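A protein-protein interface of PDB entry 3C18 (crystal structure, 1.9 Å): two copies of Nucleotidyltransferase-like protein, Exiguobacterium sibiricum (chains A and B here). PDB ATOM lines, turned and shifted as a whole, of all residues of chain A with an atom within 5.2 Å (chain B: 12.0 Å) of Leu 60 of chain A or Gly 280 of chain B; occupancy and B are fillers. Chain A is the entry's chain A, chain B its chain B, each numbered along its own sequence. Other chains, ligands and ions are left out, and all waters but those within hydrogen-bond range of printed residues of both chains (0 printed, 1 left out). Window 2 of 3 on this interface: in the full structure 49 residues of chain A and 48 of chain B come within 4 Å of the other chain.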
ATOM      1  N   ALA A   5      19.973   5.639  13.106  1.00  0.00           N
ATOM      2  CA  ALA A   5      18.595   5.978  13.549  1.00  0.00           C
ATOM      3  C   ALA A   5      17.939   4.879  14.393  1.00  0.00           C
ATOM      4  O   ALA A   5      16.927   5.114  15.069  1.00  0.00           O
ATOM      5  CB  ALA A   5      17.703   6.311  12.358  1.00  0.00           C
ATOM      6  N   THR A   6      18.523   3.685  14.358  1.00  0.00           N
ATOM      7  CA  THR A   6      17.956   2.527  15.101  1.00  0.00           C
ATOM      8  C   THR A   6      18.924   1.935  16.130  1.00  0.00           C
ATOM      9  O   THR A   6      18.649   0.908  16.770  1.00  0.00           O
ATOM     10  CB  THR A   6      17.525   1.377  14.156  1.00  0.00           C
ATOM     11  OG1 THR A   6      18.672   0.826  13.513  1.00  0.00           O
ATOM     12  CG2 THR A   6      16.552   1.856  13.102  1.00  0.00           C
ATOM     13  N   THR A   8      19.804   2.563  19.059  1.00  0.00           N
ATOM     14  CA  THR A   8      19.321   2.405  20.434  1.00  0.00           C
ATOM     15  C   THR A   8      18.459   1.160  20.552  1.00  0.00           C
ATOM     16  O   THR A   8      18.257   0.611  21.644  1.00  0.00           O
ATOM     17  CB  THR A   8      18.526   3.645  20.891  1.00  0.00           C
ATOM     18  OG1 THR A   8      19.410   4.769  20.985  1.00  0.00           O
ATOM     19  CG2 THR A   8      17.873   3.409  22.237  1.00  0.00           C
ATOM     20  N   ILE A   9      17.963   0.710  19.414  1.00  0.00           N
ATOM     21  CA  ILE A   9      17.102  -0.476  19.382  1.00  0.00           C
ATOM     22  C   ILE A   9      17.902  -1.747  19.085  1.00  0.00           C
ATOM     23  O   ILE A   9      17.747  -2.744  19.755  1.00  0.00           O
ATOM     24  CB  ILE A   9      15.944  -0.350  18.351  1.00  0.00           C
ATOM     25  CG1 ILE A   9      15.019   0.811  18.725  1.00  0.00           C
ATOM     26  CG2 ILE A   9      15.142  -1.681  18.267  1.00  0.00           C
ATOM     27  CD1 ILE A   9      13.799   0.985  17.836  1.00  0.00           C
ATOM     28  N   TYR A  58       8.274  -0.712  17.881  1.00  0.00           N
ATOM     29  CA  TYR A  58       8.849   0.429  18.571  1.00  0.00           C
ATOM     30  C   TYR A  58       8.607   1.753  17.863  1.00  0.00           C
ATOM     31  O   TYR A  58       8.392   1.807  16.660  1.00  0.00           O
ATOM     32  CB  TYR A  58      10.379   0.275  18.592  1.00  0.00           C
ATOM     33  CG  TYR A  58      10.880  -0.992  19.242  1.00  0.00           C
ATOM     34  CD1 TYR A  58      10.946  -1.106  20.630  1.00  0.00           C
ATOM     35  CD2 TYR A  58      11.304  -2.073  18.470  1.00  0.00           C
ATOM     36  CE1 TYR A  58      11.402  -2.257  21.218  1.00  0.00           C
ATOM     37  CE2 TYR A  58      11.770  -3.230  19.057  1.00  0.00           C
ATOM     38  CZ  TYR A  58      11.809  -3.312  20.424  1.00  0.00           C
ATOM     39  OH  TYR A  58      12.271  -4.455  21.009  1.00  0.00           O
ATOM     40  N   ARG A  59       8.648   2.823  18.641  1.00  0.00           N
ATOM     41  CA  ARG A  59       8.808   4.190  18.084  1.00  0.00           C
ATOM     42  C   ARG A  59      10.008   4.837  18.777  1.00  0.00           C
ATOM     43  O   ARG A  59      10.143   4.829  20.006  1.00  0.00           O
ATOM     44  CB  ARG A  59       7.566   5.078  18.202  1.00  0.00           C
ATOM     45  CG  ARG A  59       7.675   6.320  17.310  1.00  0.00           C
ATOM     46  CD  ARG A  59       6.391   7.109  17.290  1.00  0.00           C
ATOM     47  NE  ARG A  59       6.089   7.683  18.582  1.00  0.00           N
ATOM     48  CZ  ARG A  59       4.954   8.304  18.863  1.00  0.00           C
ATOM     49  NH1 ARG A  59       4.022   8.425  17.940  1.00  0.00           N
ATOM     50  NH2 ARG A  59       4.738   8.791  20.067  1.00  0.00           N
ATOM     51  N   LEU A  60      10.936   5.302  17.966  1.00  0.00           N
ATOM     52  CA  LEU A  60      12.114   5.965  18.493  1.00  0.00           C
ATOM     53  C   LEU A  60      12.124   7.355  17.913  1.00  0.00           C
ATOM     54  O   LEU A  60      12.437   7.585  16.727  1.00  0.00           O
ATOM     55  CB  LEU A  60      13.414   5.214  18.208  1.00  0.00           C
ATOM     56  CG  LEU A  60      14.627   5.943  18.795  1.00  0.00           C
ATOM     57  CD1 LEU A  60      14.440   6.312  20.278  1.00  0.00           C
ATOM     58  CD2 LEU A  60      15.899   5.151  18.585  1.00  0.00           C
ATOM     59  N   ASN A  61      11.746   8.269  18.794  1.00  0.00           N
ATOM     60  CA  ASN A  61      11.541   9.645  18.453  1.00  0.00           C
ATOM     61  C   ASN A  61      10.315   9.689  17.571  1.00  0.00           C
ATOM     62  O   ASN A  61       9.168   9.566  18.045  1.00  0.00           O
ATOM     63  CB  ASN A  61      12.781  10.230  17.790  1.00  0.00           C
ATOM     64  CG  ASN A  61      13.966  10.317  18.784  1.00  0.00           C
ATOM     65  OD1 ASN A  61      13.760  10.500  19.996  1.00  0.00           O
ATOM     66  ND2 ASN A  61      15.189  10.157  18.286  1.00  0.00           N
ATOM     67  N   THR A  62      10.564   9.805  16.290  1.00  0.00           N
ATOM     68  CA  THR A  62       9.464   9.914  15.351  1.00  0.00           C
ATOM     69  C   THR A  62       9.364   8.660  14.464  1.00  0.00           C
ATOM     70  O   THR A  62       8.367   8.422  13.764  1.00  0.00           O
ATOM     71  CB  THR A  62       9.654  11.197  14.505  1.00  0.00           C
ATOM     72  OG1 THR A  62       8.595  11.294  13.555  1.00  0.00           O
ATOM     73  CG2 THR A  62      11.002  11.192  13.751  1.00  0.00           C
ATOM     74  N   LEU A  63      10.425   7.859  14.542  1.00  0.00           N
ATOM     75  CA  LEU A  63      10.632   6.703  13.658  1.00  0.00           C
ATOM     76  C   LEU A  63      10.036   5.430  14.201  1.00  0.00           C
ATOM     77  O   LEU A  63      10.443   4.950  15.243  1.00  0.00           O
ATOM     78  CB  LEU A  63      12.128   6.483  13.418  1.00  0.00           C
ATOM     79  CG  LEU A  63      12.469   5.490  12.300  1.00  0.00           C
ATOM     80  CD1 LEU A  63      12.116   6.087  10.927  1.00  0.00           C
ATOM     81  CD2 LEU A  63      13.926   5.092  12.343  1.00  0.00           C
ATOM     82  N   ARG A  64       9.073   4.897  13.464  1.00  0.00           N
ATOM     83  CA  ARG A  64       8.391   3.643  13.816  1.00  0.00           C
ATOM     84  C   ARG A  64       9.122   2.479  13.203  1.00  0.00           C
ATOM     85  O   ARG A  64       9.378   2.429  12.000  1.00  0.00           O
ATOM     86  CB  ARG A  64       6.939   3.647  13.347  1.00  0.00           C
ATOM     87  CG  ARG A  64       6.126   4.725  13.974  1.00  0.00           C
ATOM     88  CD  ARG A  64       4.859   4.976  13.208  1.00  0.00           C
ATOM     89  NE  ARG A  64       3.756   4.133  13.646  1.00  0.00           N
ATOM     90  CZ  ARG A  64       2.670   3.884  12.917  1.00  0.00           C
ATOM     91  NH1 ARG A  64       2.550   4.395  11.697  1.00  0.00           N
ATOM     92  NH2 ARG A  64       1.713   3.101  13.397  1.00  0.00           N
ATOM     93  N   ILE B 271      -4.325   2.478  18.821  1.00  0.00           N
ATOM     94  CA  ILE B 271      -2.847   2.464  18.856  1.00  0.00           C
ATOM     95  C   ILE B 271      -2.336   3.639  19.671  1.00  0.00           C
ATOM     96  O   ILE B 271      -2.807   4.778  19.536  1.00  0.00           O
ATOM     97  CB  ILE B 271      -2.213   2.527  17.438  1.00  0.00           C
ATOM     98  CG1 ILE B 271      -0.709   2.246  17.523  1.00  0.00           C
ATOM     99  CG2 ILE B 271      -2.440   3.891  16.814  1.00  0.00           C
ATOM    100  CD1 ILE B 271      -0.051   2.058  16.191  1.00  0.00           C
ATOM    101  N   SER B 272      -1.399   3.334  20.561  1.00  0.00           N
ATOM    102  CA  SER B 272      -0.742   4.340  21.373  1.00  0.00           C
ATOM    103  C   SER B 272       0.728   4.053  21.502  1.00  0.00           C
ATOM    104  O   SER B 272       1.252   3.117  20.930  1.00  0.00           O
ATOM    105  CB  SER B 272      -1.384   4.470  22.752  1.00  0.00           C
ATOM    106  OG  SER B 272      -1.476   3.206  23.393  1.00  0.00           O
ATOM    107  N   TYR B 273       1.400   4.882  22.262  1.00  0.00           N
ATOM    108  CA  TYR B 273       2.849   4.765  22.395  1.00  0.00           C
ATOM    109  C   TYR B 273       3.251   5.004  23.812  1.00  0.00           C
ATOM    110  O   TYR B 273       2.897   6.026  24.384  1.00  0.00           O
ATOM    111  CB  TYR B 273       3.545   5.733  21.433  1.00  0.00           C
ATOM    112  CG  TYR B 273       3.143   5.540  19.984  1.00  0.00           C
ATOM    113  CD1 TYR B 273       2.045   6.195  19.452  1.00  0.00           C
ATOM    114  CD2 TYR B 273       3.851   4.685  19.164  1.00  0.00           C
ATOM    115  CE1 TYR B 273       1.682   6.012  18.139  1.00  0.00           C
ATOM    116  CE2 TYR B 273       3.512   4.498  17.860  1.00  0.00           C
ATOM    117  CZ  TYR B 273       2.410   5.156  17.346  1.00  0.00           C
ATOM    118  OH  TYR B 273       2.061   4.963  16.034  1.00  0.00           O
ATOM    119  N   GLN B 274       3.969   4.032  24.392  1.00  0.00           N
ATOM    120  CA  GLN B 274       4.401   4.106  25.786  1.00  0.00           C
ATOM    121  C   GLN B 274       5.901   4.172  25.902  1.00  0.00           C
ATOM    122  O   GLN B 274       6.592   3.217  25.621  1.00  0.00           O
ATOM    123  CB  GLN B 274       3.878   2.902  26.596  1.00  0.00           C
ATOM    124  CG  GLN B 274       2.362   2.913  26.835  1.00  0.00           C
ATOM    125  CD  GLN B 274       1.849   1.735  27.678  1.00  0.00           C
ATOM    126  OE1 GLN B 274       2.570   0.774  27.952  1.00  0.00           O
ATOM    127  NE2 GLN B 274       0.586   1.809  28.071  1.00  0.00           N
ATOM    128  N   ARG B 275       6.391   5.312  26.354  1.00  0.00           N
ATOM    129  CA  ARG B 275       7.831   5.477  26.530  1.00  0.00           C
ATOM    130  C   ARG B 275       8.280   4.877  27.847  1.00  0.00           C
ATOM    131  O   ARG B 275       7.712   5.131  28.909  1.00  0.00           O
ATOM    132  CB  ARG B 275       8.244   6.949  26.481  1.00  0.00           C
ATOM    133  CG  ARG B 275       9.769   7.141  26.427  1.00  0.00           C
ATOM    134  CD  ARG B 275      10.135   8.579  26.106  1.00  0.00           C
ATOM    135  NE  ARG B 275       9.696   9.493  27.152  1.00  0.00           N
ATOM    136  CZ  ARG B 275      10.273   9.580  28.346  1.00  0.00           C
ATOM    137  NH1 ARG B 275      11.292   8.795  28.637  1.00  0.00           N
ATOM    138  NH2 ARG B 275       9.843  10.437  29.242  1.00  0.00           N
ATOM    139  N   THR B 276       9.349   4.110  27.764  1.00  0.00           N
ATOM    140  CA  THR B 276       9.962   3.503  28.947  1.00  0.00           C
ATOM    141  C   THR B 276      10.677   4.509  29.805  1.00  0.00           C
ATOM    142  O   THR B 276      11.507   5.279  29.328  1.00  0.00           O
ATOM    143  CB  THR B 276      10.946   2.443  28.560  1.00  0.00           C
ATOM    144  OG1 THR B 276      10.265   1.487  27.750  1.00  0.00           O
ATOM    145  CG2 THR B 276      11.532   1.732  29.790  1.00  0.00           C
ATOM    146  N   LYS B 277      10.358   4.459  31.101  1.00  0.00           N
ATOM    147  CA  LYS B 277      10.937   5.359  32.073  1.00  0.00           C
ATOM    148  C   LYS B 277      12.436   5.263  32.040  1.00  0.00           C
ATOM    149  O   LYS B 277      13.006   4.181  32.163  1.00  0.00           O
ATOM    150  CB  LYS B 277      10.402   5.107  33.493  1.00  0.00           C
ATOM    151  CG  LYS B 277       9.004   5.667  33.709  1.00  0.00           C
ATOM    152  CD  LYS B 277       8.527   5.595  35.168  1.00  0.00           C
ATOM    153  CE  LYS B 277       7.094   6.086  35.316  1.00  0.00           C
ATOM    154  NZ  LYS B 277       6.833   6.181  36.780  1.00  0.00           N
ATOM    155  N   GLY B 278      13.047   6.430  31.862  1.00  0.00           N
ATOM    156  CA  GLY B 278      14.500   6.571  31.838  1.00  0.00           C
ATOM    157  C   GLY B 278      15.122   6.376  30.471  1.00  0.00           C
ATOM    158  O   GLY B 278      16.337   6.536  30.292  1.00  0.00           O
ATOM    159  N   LEU B 279      14.282   6.028  29.504  1.00  0.00           N
ATOM    160  CA  LEU B 279      14.762   5.718  28.138  1.00  0.00           C
ATOM    161  C   LEU B 279      14.028   6.492  27.079  1.00  0.00           C
ATOM    162  O   LEU B 279      12.965   7.059  27.321  1.00  0.00           O
ATOM    163  CB  LEU B 279      14.655   4.230  27.833  1.00  0.00           C
ATOM    164  CG  LEU B 279      15.423   3.322  28.789  1.00  0.00           C
ATOM    165  CD1 LEU B 279      15.060   1.863  28.561  1.00  0.00           C
ATOM    166  CD2 LEU B 279      16.922   3.534  28.629  1.00  0.00           C
ATOM    167  N   GLY B 280      14.576   6.440  25.871  1.00  0.00           N
ATOM    168  CA  GLY B 280      14.003   7.198  24.732  1.00  0.00           C
ATOM    169  C   GLY B 280      13.034   6.424  23.873  1.00  0.00           C
ATOM    170  O   GLY B 280      12.132   6.979  23.263  1.00  0.00           O
ATOM    171  N   VAL B 281      13.235   5.126  23.845  1.00  0.00           N
ATOM    172  CA  VAL B 281      12.405   4.227  23.051  1.00  0.00           C
ATOM    173  C   VAL B 281      10.991   4.092  23.603  1.00  0.00           C
ATOM    174  O   VAL B 281      10.783   4.006  24.792  1.00  0.00           O
ATOM    175  CB  VAL B 281      13.027   2.840  22.937  1.00  0.00           C
ATOM    176  CG1 VAL B 281      12.892   2.105  24.288  1.00  0.00           C
ATOM    177  CG2 VAL B 281      12.360   2.072  21.821  1.00  0.00           C
ATOM    178  N   GLU B 282      10.032   4.137  22.691  1.00  0.00           N
ATOM    179  CA  GLU B 282       8.644   3.858  22.999  1.00  0.00           C
ATOM    180  C   GLU B 282       8.211   2.501  22.446  1.00  0.00           C
ATOM    181  O   GLU B 282       8.629   2.062  21.366  1.00  0.00           O
ATOM    182  CB  GLU B 282       7.742   4.903  22.379  1.00  0.00           C
ATOM    183  CG  GLU B 282       7.813   6.269  23.008  1.00  0.00           C
ATOM    184  CD  GLU B 282       7.362   7.353  22.044  1.00  0.00           C
ATOM    185  OE1 GLU B 282       7.967   7.468  20.945  1.00  0.00           O
ATOM    186  OE2 GLU B 282       6.421   8.089  22.386  1.00  0.00           O
ATOM    187  N   LEU B 283       7.345   1.840  23.200  1.00  0.00           N
ATOM    188  CA  LEU B 283       6.713   0.619  22.718  1.00  0.00           C
ATOM    189  C   LEU B 283       5.354   0.986  22.201  1.00  0.00           C
ATOM    190  O   LEU B 283       4.633   1.731  22.837  1.00  0.00           O
ATOM    191  CB  LEU B 283       6.606  -0.435  23.824  1.00  0.00           C
ATOM    192  CG  LEU B 283       7.952  -1.074  24.214  1.00  0.00           C
ATOM    193  CD1 LEU B 283       7.821  -1.889  25.468  1.00  0.00           C
ATOM    194  CD2 LEU B 283       8.470  -1.937  23.110  1.00  0.00           C
ATOM    195  N   VAL B 284       5.013   0.457  21.028  1.00  0.00           N
ATOM    196  CA  VAL B 284       3.692   0.701  20.430  1.00  0.00           C
ATOM    197  C   VAL B 284       2.736  -0.208  21.177  1.00  0.00           C
ATOM    198  O   VAL B 284       3.035  -1.375  21.441  1.00  0.00           O
ATOM    199  CB  VAL B 284       3.665   0.444  18.893  1.00  0.00           C
ATOM    200  CG1 VAL B 284       2.323   0.865  18.293  1.00  0.00           C
ATOM    201  CG2 VAL B 284       4.785   1.207  18.218  1.00  0.00           C
ATOM    202  N   THR B 285       1.607   0.336  21.583  1.00  0.00           N
ATOM    203  CA  THR B 285       0.639  -0.445  22.350  1.00  0.00           C
ATOM    204  C   THR B 285      -0.701  -0.459  21.647  1.00  0.00           C
ATOM    205  O   THR B 285      -1.033   0.426  20.859  1.00  0.00           O
ATOM    206  CB  THR B 285       0.516   0.048  23.808  1.00  0.00           C
ATOM    207  OG1 THR B 285       0.271   1.446  23.808  1.00  0.00           O
ATOM    208  CG2 THR B 285       1.804  -0.211  24.592  1.00  0.00           C
ATOM    209  N   TYR B 286      -1.446  -1.518  21.906  1.00  0.00           N
ATOM    210  CA  TYR B 286      -2.716  -1.749  21.209  1.00  0.00           C
ATOM    211  C   TYR B 286      -3.781  -2.127  22.192  1.00  0.00           C
ATOM    212  O   TYR B 286      -3.555  -2.923  23.084  1.00  0.00           O
ATOM    213  CB  TYR B 286      -2.561  -2.876  20.175  1.00  0.00           C
ATOM    214  CG  TYR B 286      -1.472  -2.610  19.151  1.00  0.00           C
ATOM    215  CD1 TYR B 286      -1.707  -1.796  18.062  1.00  0.00           C
ATOM    216  CD2 TYR B 286      -0.206  -3.164  19.287  1.00  0.00           C
ATOM    217  CE1 TYR B 286      -0.728  -1.534  17.135  1.00  0.00           C
ATOM    218  CE2 TYR B 286       0.793  -2.884  18.360  1.00  0.00           C
ATOM    219  CZ  TYR B 286       0.514  -2.073  17.296  1.00  0.00           C
ATOM    220  OH  TYR B 286       1.471  -1.807  16.370  1.00  0.00           O
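Hydrophobic or aromatic side chains of chain A that line the printed part of chain B: Tyr 58 and Leu 60.
Along chain A the printed residues that touch a printed residue of chain B span positions 58 to 64.
Printed residues of chain B that touch a printed residue of chain A: Ile 271, Tyr 273, Gly 280, Val 281, Glu 282, Leu 283 and Val 284.
Hydrophobic or aromatic side chains of chain B within 4 Å of the printed part of chain A: Ile 271, Tyr 273, Val 281, Leu 283 and Val 284.
Among the printed residues, Asp or Glu carboxylates within 4 Å of a Lys or Arg side-chain nitrogen of the other chain: Arg 59 of chain A with Glu 282 of chain B (3.0 Å).
Ala 5 of chain A touches none of the printed residues of chain B.
Thr 6 of chain A touches none of the printed residues of chain B.
Leu 60 of chain A touches just these residues of chain B: Gly 280 (3.8 Å) and Val 281 (3.9 Å).
No residue of chain B comes within 4 Å of Thr 62 of chain A.
No residue of chain B comes within 4 Å of Leu 63 of chain A.
Of the printed residues of chain B, Arg 64 of chain A touches Ile 271 (3.5 Å) and Tyr 273 (3.0 Å).
Gly 280 of chain B touches just one residue of chain A: Leu 60.
Printed residues of chain A within 4 Å of Val 281 of chain B: Tyr 58, Arg 59 and Leu 60.
Of the printed residues of chain A, Glu 282 of chain B touches Tyr 58, Arg 59 and Asn 61.
Of the printed residues of chain A, Leu 283 of chain B touches Tyr 58 (3.5 Å).
The nearest residue of chain A that does not touch Gly 280 of chain B is Arg 59 of chain A (4.4 Å).
The nearest printed residue of chain A that does not touch Glu 282 of chain B is Leu 60 of chain A (4.7 Å).
The backbone NH of Thr 276 of chain B is in hydrogen-bond range of the backbone carbonyl oxygen of Val 281 of chain B, at 3.3 Å.
The backbone NH (N) of Gln 274 of chain B sits at hydrogen-bond distance from the backbone carbonyl oxygen (O) of Leu 283 of chain B (2.9 Å).
Among the printed residues, pairs that only touch across the chains: Tyr 58 of chain A with Glu 282 of chain B, Arg 59 of chain A with Tyr 273 of chain B, Arg 64 of chain A with Ile 271 of chain B, Tyr 58 of chain A with Leu 283 of chain B, Tyr 58 of chain A with Val 281 of chain B, Arg 59 of chain A with Val 281 of chain B, Asn 61 of chain A with Glu 282 of chain B, Leu 60 of chain A with Gly 280 of chain B, Tyr 58 of chain A with Val 284 of chain B and Leu 60 of chain A with Val 281 of chain B.
No position is printed for both chains.
Of the 12 pairs that touch across the chains among the printed residues, none has its exchanged pair printed and touching as well.
NE of Arg 64 of chain A lies within hydrogen-bond range of OH of Tyr 273 of chain B (3.0 Å).
The guanidinium group (NH2) of Arg 59 of chain A lies within salt-bridge range of the side-chain carboxylate (OE2) of Glu 282 of chain B.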
